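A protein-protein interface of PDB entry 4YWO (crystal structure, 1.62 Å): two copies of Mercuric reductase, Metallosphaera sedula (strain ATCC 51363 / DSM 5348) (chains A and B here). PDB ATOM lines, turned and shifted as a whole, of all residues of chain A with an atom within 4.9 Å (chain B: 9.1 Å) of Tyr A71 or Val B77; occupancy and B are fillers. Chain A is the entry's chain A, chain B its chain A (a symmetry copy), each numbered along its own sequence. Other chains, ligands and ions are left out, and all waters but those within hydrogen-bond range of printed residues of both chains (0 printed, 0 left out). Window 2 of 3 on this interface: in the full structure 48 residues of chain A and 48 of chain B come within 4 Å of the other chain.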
ATOM      1  N   ILE A  67     -25.983   0.374  23.780  1.00  0.00           N
ATOM      2  CA  ILE A  67     -24.910   0.326  24.841  1.00  0.00           C
ATOM      3  C   ILE A  67     -24.266  -1.030  24.828  1.00  0.00           C
ATOM      4  O   ILE A  67     -23.004  -1.141  24.843  1.00  0.00           O
ATOM      5  CB  ILE A  67     -25.518   0.580  26.209  1.00  0.00           C
ATOM      6  CG1 ILE A  67     -25.898   2.019  26.244  1.00  0.00           C
ATOM      7  CG2 ILE A  67     -24.409   0.375  27.269  1.00  0.00           C
ATOM      8  CD1 ILE A  67     -26.636   2.355  27.447  1.00  0.00           C
ATOM      9  N   ALA A  68     -25.037  -2.105  24.749  1.00  0.00           N
ATOM     10  CA  ALA A  68     -24.517  -3.441  24.674  1.00  0.00           C
ATOM     11  C   ALA A  68     -23.522  -3.607  23.461  1.00  0.00           C
ATOM     12  O   ALA A  68     -22.493  -4.277  23.565  1.00  0.00           O
ATOM     13  CB  ALA A  68     -25.530  -4.493  24.669  1.00  0.00           C
ATOM     14  N   GLU A  69     -23.972  -3.152  22.319  1.00  0.00           N
ATOM     15  CA  GLU A  69     -23.214  -3.222  21.106  1.00  0.00           C
ATOM     16  C   GLU A  69     -21.870  -2.482  21.175  1.00  0.00           C
ATOM     17  O   GLU A  69     -20.845  -3.014  20.714  1.00  0.00           O
ATOM     18  CB  GLU A  69     -24.047  -2.716  19.910  1.00  0.00           C
ATOM     19  CG  GLU A  69     -23.238  -2.618  18.631  1.00  0.00           C
ATOM     20  CD  GLU A  69     -22.623  -1.208  18.284  1.00  0.00           C
ATOM     21  OE1 GLU A  69     -23.340  -0.154  18.407  1.00  0.00           O
ATOM     22  OE2 GLU A  69     -21.408  -1.170  17.787  1.00  0.00           O
ATOM     23  N   ILE A  70     -21.838  -1.283  21.654  1.00  0.00           N
ATOM     24  CA  ILE A  70     -20.572  -0.507  21.609  1.00  0.00           C
ATOM     25  C   ILE A  70     -19.561  -1.116  22.586  1.00  0.00           C
ATOM     26  O   ILE A  70     -18.392  -1.160  22.312  1.00  0.00           O
ATOM     27  CB  ILE A  70     -20.742   0.991  21.839  1.00  0.00           C
ATOM     28  CG1 ILE A  70     -21.314   1.332  23.207  1.00  0.00           C
ATOM     29  CG2 ILE A  70     -21.640   1.582  20.744  1.00  0.00           C
ATOM     30  CD1 ILE A  70     -21.508   2.790  23.484  1.00  0.00           C
ATOM     31  N   TYR A  71     -20.059  -1.643  23.698  1.00  0.00           N
ATOM     32  CA  TYR A  71     -19.115  -2.316  24.623  1.00  0.00           C
ATOM     33  C   TYR A  71     -18.627  -3.596  24.051  1.00  0.00           C
ATOM     34  O   TYR A  71     -17.396  -3.959  24.287  1.00  0.00           O
ATOM     35  CB  TYR A  71     -19.721  -2.542  26.061  1.00  0.00           C
ATOM     36  CG  TYR A  71     -19.648  -1.367  26.938  1.00  0.00           C
ATOM     37  CD1 TYR A  71     -20.522  -0.305  26.838  1.00  0.00           C
ATOM     38  CD2 TYR A  71     -18.687  -1.282  27.964  1.00  0.00           C
ATOM     39  CE1 TYR A  71     -20.422   0.831  27.620  1.00  0.00           C
ATOM     40  CE2 TYR A  71     -18.618  -0.158  28.748  1.00  0.00           C
ATOM     41  CZ  TYR A  71     -19.405   0.876  28.623  1.00  0.00           C
ATOM     42  OH  TYR A  71     -19.344   2.028  29.390  1.00  0.00           O
ATOM     43  N   LYS A  72     -19.467  -4.386  23.372  1.00  0.00           N
ATOM     44  CA  LYS A  72     -19.051  -5.616  22.728  1.00  0.00           C
ATOM     45  C   LYS A  72     -17.935  -5.291  21.725  1.00  0.00           C
ATOM     46  O   LYS A  72     -16.911  -5.995  21.690  1.00  0.00           O
ATOM     47  CB  LYS A  72     -20.220  -6.345  22.052  1.00  0.00           C
ATOM     48  CG  LYS A  72     -19.741  -7.583  21.285  1.00  0.00           C
ATOM     49  CD  LYS A  72     -20.619  -8.770  21.273  1.00  0.00           C
ATOM     50  CE  LYS A  72     -20.061 -10.059  20.570  1.00  0.00           C
ATOM     51  NZ  LYS A  72     -18.942 -10.584  21.334  1.00  0.00           N
ATOM     52  N   LYS A  73     -18.137  -4.274  20.919  1.00  0.00           N
ATOM     53  CA  LYS A  73     -17.090  -3.917  19.926  1.00  0.00           C
ATOM     54  C   LYS A  73     -15.825  -3.532  20.612  1.00  0.00           C
ATOM     55  O   LYS A  73     -14.717  -3.909  20.160  1.00  0.00           O
ATOM     56  CB  LYS A  73     -17.559  -2.962  18.832  1.00  0.00           C
ATOM     57  CG  LYS A  73     -16.581  -2.970  17.658  1.00  0.00           C
ATOM     58  CD  LYS A  73     -16.626  -4.318  16.940  1.00  0.00           C
ATOM     59  CE  LYS A  73     -15.695  -4.406  15.783  1.00  0.00           C
ATOM     60  NZ  LYS A  73     -15.749  -5.831  15.360  1.00  0.00           N
ATOM     61  N   ALA A  74     -15.951  -2.714  21.635  1.00  0.00           N
ATOM     62  CA  ALA A  74     -14.760  -2.334  22.431  1.00  0.00           C
ATOM     63  C   ALA A  74     -13.994  -3.545  22.979  1.00  0.00           C
ATOM     64  O   ALA A  74     -12.714  -3.539  22.949  1.00  0.00           O
ATOM     65  CB  ALA A  74     -15.105  -1.362  23.516  1.00  0.00           C
ATOM     66  N   ARG A  75     -14.695  -4.595  23.425  1.00  0.00           N
ATOM     67  CA  ARG A  75     -14.026  -5.855  23.910  1.00  0.00           C
ATOM     68  C   ARG A  75     -13.392  -6.567  22.781  1.00  0.00           C
ATOM     69  O   ARG A  75     -12.284  -7.105  22.912  1.00  0.00           O
ATOM     70  CB  ARG A  75     -15.024  -6.863  24.461  1.00  0.00           C
ATOM     71  CG  ARG A  75     -15.541  -6.447  25.784  1.00  0.00           C
ATOM     72  CD  ARG A  75     -16.209  -7.607  26.480  1.00  0.00           C
ATOM     73  NE  ARG A  75     -17.427  -8.130  25.916  1.00  0.00           N
ATOM     74  CZ  ARG A  75     -18.597  -7.492  25.937  1.00  0.00           C
ATOM     75  NH1 ARG A  75     -18.716  -6.274  26.467  1.00  0.00           N
ATOM     76  NH2 ARG A  75     -19.631  -8.090  25.377  1.00  0.00           N
ATOM     77  N   VAL A  82     -14.358  -5.362  29.268  1.00  0.00           N
ATOM     78  CA  VAL A  82     -15.133  -4.247  29.665  1.00  0.00           C
ATOM     79  C   VAL A  82     -16.627  -4.479  29.237  1.00  0.00           C
ATOM     80  O   VAL A  82     -16.875  -4.774  28.115  1.00  0.00           O
ATOM     81  CB  VAL A  82     -14.535  -3.031  29.046  1.00  0.00           C
ATOM     82  CG1 VAL A  82     -14.525  -3.154  27.507  1.00  0.00           C
ATOM     83  CG2 VAL A  82     -15.221  -1.805  29.490  1.00  0.00           C
ATOM     84  N   TYR A  83     -17.496  -4.537  30.243  1.00  0.00           N
ATOM     85  CA  TYR A  83     -18.969  -4.649  30.061  1.00  0.00           C
ATOM     86  C   TYR A  83     -19.654  -3.344  30.482  1.00  0.00           C
ATOM     87  O   TYR A  83     -19.174  -2.552  31.277  1.00  0.00           O
ATOM     88  CB  TYR A  83     -19.480  -5.869  30.834  1.00  0.00           C
ATOM     89  CG  TYR A  83     -19.004  -7.159  30.244  1.00  0.00           C
ATOM     90  CD1 TYR A  83     -17.775  -7.701  30.640  1.00  0.00           C
ATOM     91  CD2 TYR A  83     -19.730  -7.830  29.333  1.00  0.00           C
ATOM     92  CE1 TYR A  83     -17.314  -8.864  30.092  1.00  0.00           C
ATOM     93  CE2 TYR A  83     -19.265  -9.027  28.783  1.00  0.00           C
ATOM     94  CZ  TYR A  83     -18.054  -9.501  29.173  1.00  0.00           C
ATOM     95  OH  TYR A  83     -17.665 -10.684  28.617  1.00  0.00           O
ATOM     96  N   PRO A  84     -20.869  -3.127  29.972  1.00  0.00           N
ATOM     97  CA  PRO A  84     -21.538  -1.931  30.330  1.00  0.00           C
ATOM     98  C   PRO A  84     -21.833  -1.848  31.877  1.00  0.00           C
ATOM     99  O   PRO A  84     -22.209  -2.883  32.408  1.00  0.00           O
ATOM    100  CB  PRO A  84     -22.853  -2.070  29.626  1.00  0.00           C
ATOM    101  CG  PRO A  84     -22.604  -2.954  28.480  1.00  0.00           C
ATOM    102  CD  PRO A  84     -21.581  -3.931  28.971  1.00  0.00           C
ATOM    103  N   PRO A  85     -21.690  -0.683  32.448  1.00  0.00           N
ATOM    104  CA  PRO A  85     -21.893  -0.618  33.913  1.00  0.00           C
ATOM    105  C   PRO A  85     -23.439  -0.833  34.216  1.00  0.00           C
ATOM    106  O   PRO A  85     -24.299  -0.502  33.421  1.00  0.00           O
ATOM    107  CB  PRO A  85     -21.446   0.780  34.245  1.00  0.00           C
ATOM    108  CG  PRO A  85     -21.576   1.584  33.001  1.00  0.00           C
ATOM    109  CD  PRO A  85     -21.275   0.610  31.894  1.00  0.00           C
ATOM    110  N   GLU B  69     -12.924   3.574  12.374  1.00  0.00           N
ATOM    111  CA  GLU B  69     -14.132   3.710  13.131  1.00  0.00           C
ATOM    112  C   GLU B  69     -14.199   2.784  14.354  1.00  0.00           C
ATOM    113  O   GLU B  69     -14.603   3.226  15.444  1.00  0.00           O
ATOM    114  CB  GLU B  69     -15.368   3.504  12.232  1.00  0.00           C
ATOM    115  CG  GLU B  69     -16.666   3.477  13.015  1.00  0.00           C
ATOM    116  CD  GLU B  69     -17.224   2.059  13.421  1.00  0.00           C
ATOM    117  OE1 GLU B  69     -17.236   1.110  12.560  1.00  0.00           O
ATOM    118  OE2 GLU B  69     -17.749   1.920  14.617  1.00  0.00           O
ATOM    119  N   ILE B  70     -13.896   1.536  14.215  1.00  0.00           N
ATOM    120  CA  ILE B  70     -14.079   0.603  15.356  1.00  0.00           C
ATOM    121  C   ILE B  70     -13.049   0.916  16.446  1.00  0.00           C
ATOM    122  O   ILE B  70     -13.341   0.832  17.609  1.00  0.00           O
ATOM    123  CB  ILE B  70     -14.061  -0.873  14.973  1.00  0.00           C
ATOM    124  CG1 ILE B  70     -12.743  -1.323  14.361  1.00  0.00           C
ATOM    125  CG2 ILE B  70     -15.208  -1.166  13.997  1.00  0.00           C
ATOM    126  CD1 ILE B  70     -12.670  -2.763  13.960  1.00  0.00           C
ATOM    127  N   TYR B  71     -11.863   1.342  16.032  1.00  0.00           N
ATOM    128  CA  TYR B  71     -10.873   1.735  17.064  1.00  0.00           C
ATOM    129  C   TYR B  71     -11.268   3.002  17.730  1.00  0.00           C
ATOM    130  O   TYR B  71     -11.012   3.149  19.001  1.00  0.00           O
ATOM    131  CB  TYR B  71      -9.404   1.836  16.500  1.00  0.00           C
ATOM    132  CG  TYR B  71      -8.704   0.548  16.406  1.00  0.00           C
ATOM    133  CD1 TYR B  71      -8.934  -0.353  15.387  1.00  0.00           C
ATOM    134  CD2 TYR B  71      -7.723   0.181  17.346  1.00  0.00           C
ATOM    135  CE1 TYR B  71      -8.325  -1.592  15.325  1.00  0.00           C
ATOM    136  CE2 TYR B  71      -7.108  -1.042  17.254  1.00  0.00           C
ATOM    137  CZ  TYR B  71      -7.361  -1.924  16.327  1.00  0.00           C
ATOM    138  OH  TYR B  71      -6.767  -3.172  16.223  1.00  0.00           O
ATOM    139  N   LYS B  72     -11.810   3.992  17.011  1.00  0.00           N
ATOM    140  CA  LYS B  72     -12.281   5.230  17.598  1.00  0.00           C
ATOM    141  C   LYS B  72     -13.346   4.897  18.653  1.00  0.00           C
ATOM    142  O   LYS B  72     -13.303   5.447  19.768  1.00  0.00           O
ATOM    143  CB  LYS B  72     -12.820   6.207  16.545  1.00  0.00           C
ATOM    144  CG  LYS B  72     -13.415   7.462  17.195  1.00  0.00           C
ATOM    145  CD  LYS B  72     -13.238   8.751  16.497  1.00  0.00           C
ATOM    146  CE  LYS B  72     -13.763  10.035  17.233  1.00  0.00           C
ATOM    147  NZ  LYS B  72     -12.958  10.281  18.417  1.00  0.00           N
ATOM    148  N   LYS B  73     -14.282   4.046  18.306  1.00  0.00           N
ATOM    149  CA  LYS B  73     -15.340   3.691  19.289  1.00  0.00           C
ATOM    150  C   LYS B  73     -14.744   3.036  20.487  1.00  0.00           C
ATOM    151  O   LYS B  73     -15.163   3.312  21.636  1.00  0.00           O
ATOM    152  CB  LYS B  73     -16.547   2.979  18.685  1.00  0.00           C
ATOM    153  CG  LYS B  73     -17.730   3.017  19.652  1.00  0.00           C
ATOM    154  CD  LYS B  73     -18.249   4.446  19.800  1.00  0.00           C
ATOM    155  CE  LYS B  73     -19.402   4.567  20.731  1.00  0.00           C
ATOM    156  NZ  LYS B  73     -19.617   6.031  20.881  1.00  0.00           N
ATOM    157  N   ALA B  74     -13.845   2.105  20.246  1.00  0.00           N
ATOM    158  CA  ALA B  74     -13.138   1.449  21.373  1.00  0.00           C
ATOM    159  C   ALA B  74     -12.441   2.448  22.306  1.00  0.00           C
ATOM    160  O   ALA B  74     -12.501   2.265  23.572  1.00  0.00           O
ATOM    161  CB  ALA B  74     -12.195   0.390  20.894  1.00  0.00           C
ATOM    162  N   ARG B  75     -11.836   3.512  21.764  1.00  0.00           N
ATOM    163  CA  ARG B  75     -11.191   4.581  22.608  1.00  0.00           C
ATOM    164  C   ARG B  75     -12.223   5.351  23.335  1.00  0.00           C
ATOM    165  O   ARG B  75     -12.041   5.702  24.509  1.00  0.00           O
ATOM    166  CB  ARG B  75     -10.480   5.630  21.766  1.00  0.00           C
ATOM    167  CG  ARG B  75      -9.219   5.107  21.197  1.00  0.00           C
ATOM    168  CD  ARG B  75      -8.350   6.238  20.705  1.00  0.00           C
ATOM    169  NE  ARG B  75      -8.807   7.003  19.573  1.00  0.00           N
ATOM    170  CZ  ARG B  75      -8.850   6.542  18.324  1.00  0.00           C
ATOM    171  NH1 ARG B  75      -8.496   5.289  18.032  1.00  0.00           N
ATOM    172  NH2 ARG B  75      -9.296   7.355  17.385  1.00  0.00           N
ATOM    173  N   GLU B  76     -13.359   5.648  22.696  1.00  0.00           N
ATOM    174  CA  GLU B  76     -14.453   6.354  23.444  1.00  0.00           C
ATOM    175  C   GLU B  76     -15.006   5.582  24.574  1.00  0.00           C
ATOM    176  O   GLU B  76     -15.273   6.181  25.649  1.00  0.00           O
ATOM    177  CB  GLU B  76     -15.582   6.809  22.515  1.00  0.00           C
ATOM    178  CG  GLU B  76     -15.154   7.836  21.495  1.00  0.00           C
ATOM    179  CD  GLU B  76     -16.301   8.253  20.619  1.00  0.00           C
ATOM    180  OE1 GLU B  76     -16.050   8.583  19.460  1.00  0.00           O
ATOM    181  OE2 GLU B  76     -17.464   8.260  21.136  1.00  0.00           O
ATOM    182  N   VAL B  77     -15.196   4.289  24.438  1.00  0.00           N
ATOM    183  CA  VAL B  77     -15.829   3.450  25.444  1.00  0.00           C
ATOM    184  C   VAL B  77     -14.845   3.203  26.583  1.00  0.00           C
ATOM    185  O   VAL B  77     -15.253   3.218  27.754  1.00  0.00           O
ATOM    186  CB  VAL B  77     -16.280   2.089  24.835  1.00  0.00           C
ATOM    187  CG1 VAL B  77     -16.635   1.078  25.874  1.00  0.00           C
ATOM    188  CG2 VAL B  77     -17.476   2.375  23.857  1.00  0.00           C
ATOM    189  N   THR B  78     -13.597   2.943  26.256  1.00  0.00           N
ATOM    190  CA  THR B  78     -12.609   2.455  27.280  1.00  0.00           C
ATOM    191  C   THR B  78     -11.810   3.600  27.832  1.00  0.00           C
ATOM    192  O   THR B  78     -11.237   3.465  28.933  1.00  0.00           O
ATOM    193  CB  THR B  78     -11.617   1.405  26.724  1.00  0.00           C
ATOM    194  OG1 THR B  78     -10.875   2.020  25.657  1.00  0.00           O
ATOM    195  CG2 THR B  78     -12.213   0.188  26.238  1.00  0.00           C
ATOM    196  N   GLY B  79     -11.681   4.697  27.157  1.00  0.00           N
ATOM    197  CA  GLY B  79     -10.781   5.773  27.533  1.00  0.00           C
ATOM    198  C   GLY B  79      -9.313   5.465  27.229  1.00  0.00           C
ATOM    199  O   GLY B  79      -8.431   6.331  27.553  1.00  0.00           O
ATOM    200  N   SER B  80      -9.046   4.295  26.630  1.00  0.00           N
ATOM    201  CA  SER B  80      -7.682   3.904  26.277  1.00  0.00           C
ATOM    202  C   SER B  80      -7.246   4.570  25.006  1.00  0.00           C
ATOM    203  O   SER B  80      -8.059   5.031  24.211  1.00  0.00           O
ATOM    204  CB  SER B  80      -7.584   2.409  26.116  1.00  0.00           C
ATOM    205  OG  SER B  80      -7.911   1.823  27.340  1.00  0.00           O
ATOM    206  N   VAL B  82      -5.952   3.375  22.219  1.00  0.00           N
ATOM    207  CA  VAL B  82      -5.700   2.336  21.293  1.00  0.00           C
ATOM    208  C   VAL B  82      -6.056   2.837  19.847  1.00  0.00           C
ATOM    209  O   VAL B  82      -7.120   3.323  19.642  1.00  0.00           O
ATOM    210  CB  VAL B  82      -6.498   1.150  21.709  1.00  0.00           C
ATOM    211  CG1 VAL B  82      -8.004   1.490  21.734  1.00  0.00           C
ATOM    212  CG2 VAL B  82      -6.217  -0.018  20.854  1.00  0.00           C
ATOM    213  N   ASN B 385     -26.674   8.287  20.048  1.00  0.00           N
ATOM    214  CA  ASN B 385     -25.728   9.385  20.297  1.00  0.00           C
ATOM    215  C   ASN B 385     -25.108   9.915  19.005  1.00  0.00           C
ATOM    216  O   ASN B 385     -23.873  10.080  18.896  1.00  0.00           O
ATOM    217  CB  ASN B 385     -24.624   8.902  21.279  1.00  0.00           C
ATOM    218  CG  ASN B 385     -25.127   8.771  22.695  1.00  0.00           C
ATOM    219  OD1 ASN B 385     -26.239   9.195  23.004  1.00  0.00           O
ATOM    220  ND2 ASN B 385     -24.306   8.178  23.588  1.00  0.00           N
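The guanidinium group (NH1) of Arg A75 is in hydrogen-bond range of the backbone carbonyl oxygen (O) of Tyr A71, at 3.4 Å.
The side-chain amino group (NZ) of Lys B73 lies within salt-bridge range of the side-chain carboxylate (OE2) of Glu B76 (3.1 Å).
Among the printed residues, pairs that only touch across the chains: Ile A70 with Lys B73, Ile A70 with Val B77, Tyr A71 with Val B77, Lys A73 with Ile B70 and Ala A74 with Val B77.
Ile A70 touches just these residues of chain B: Lys B73 and Val B77.
Tyr A71 touches one residue of chain B.
Of the printed residues of chain B, Lys A73 touches Ile B70 (3.7 Å).
Printed residues of chain B within 4 Å of Ala A74: Val B77.
Printed residues of chain A within 4 Å of Ile B70: Lys A73.
Of the printed residues of chain A, Lys B73 touches Ile A70.
Val B77 touches three residues of chain A.
The nearest residue of chain B that does not touch Tyr A71 is Thr B78 (6.4 Å).
The nearest residue of chain A that does not touch Val B77 is Val A82 (4.8 Å).
The nearest printed residue of chain B that does not touch Lys A73 is Ala B74 (5.0 Å).
Of the 13 printed residues of chain A, 4 touch a printed residue of chain B.
Hydrophobic or aromatic side chains of chain A within 4 Å of the printed part of chain B: Ile A70, Tyr A71 and Ala A74.
Among the printed residues, 5 pairs touch across the chains.
Among the printed residues, no Asp or Glu carboxylate lies within 4 Å of a Lys or Arg side-chain nitrogen of the other chain.
Ile A70 touches Lys B73, and with the chains exchanged Lys A73 touches Ile B70.
8 positions are printed for both chains.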
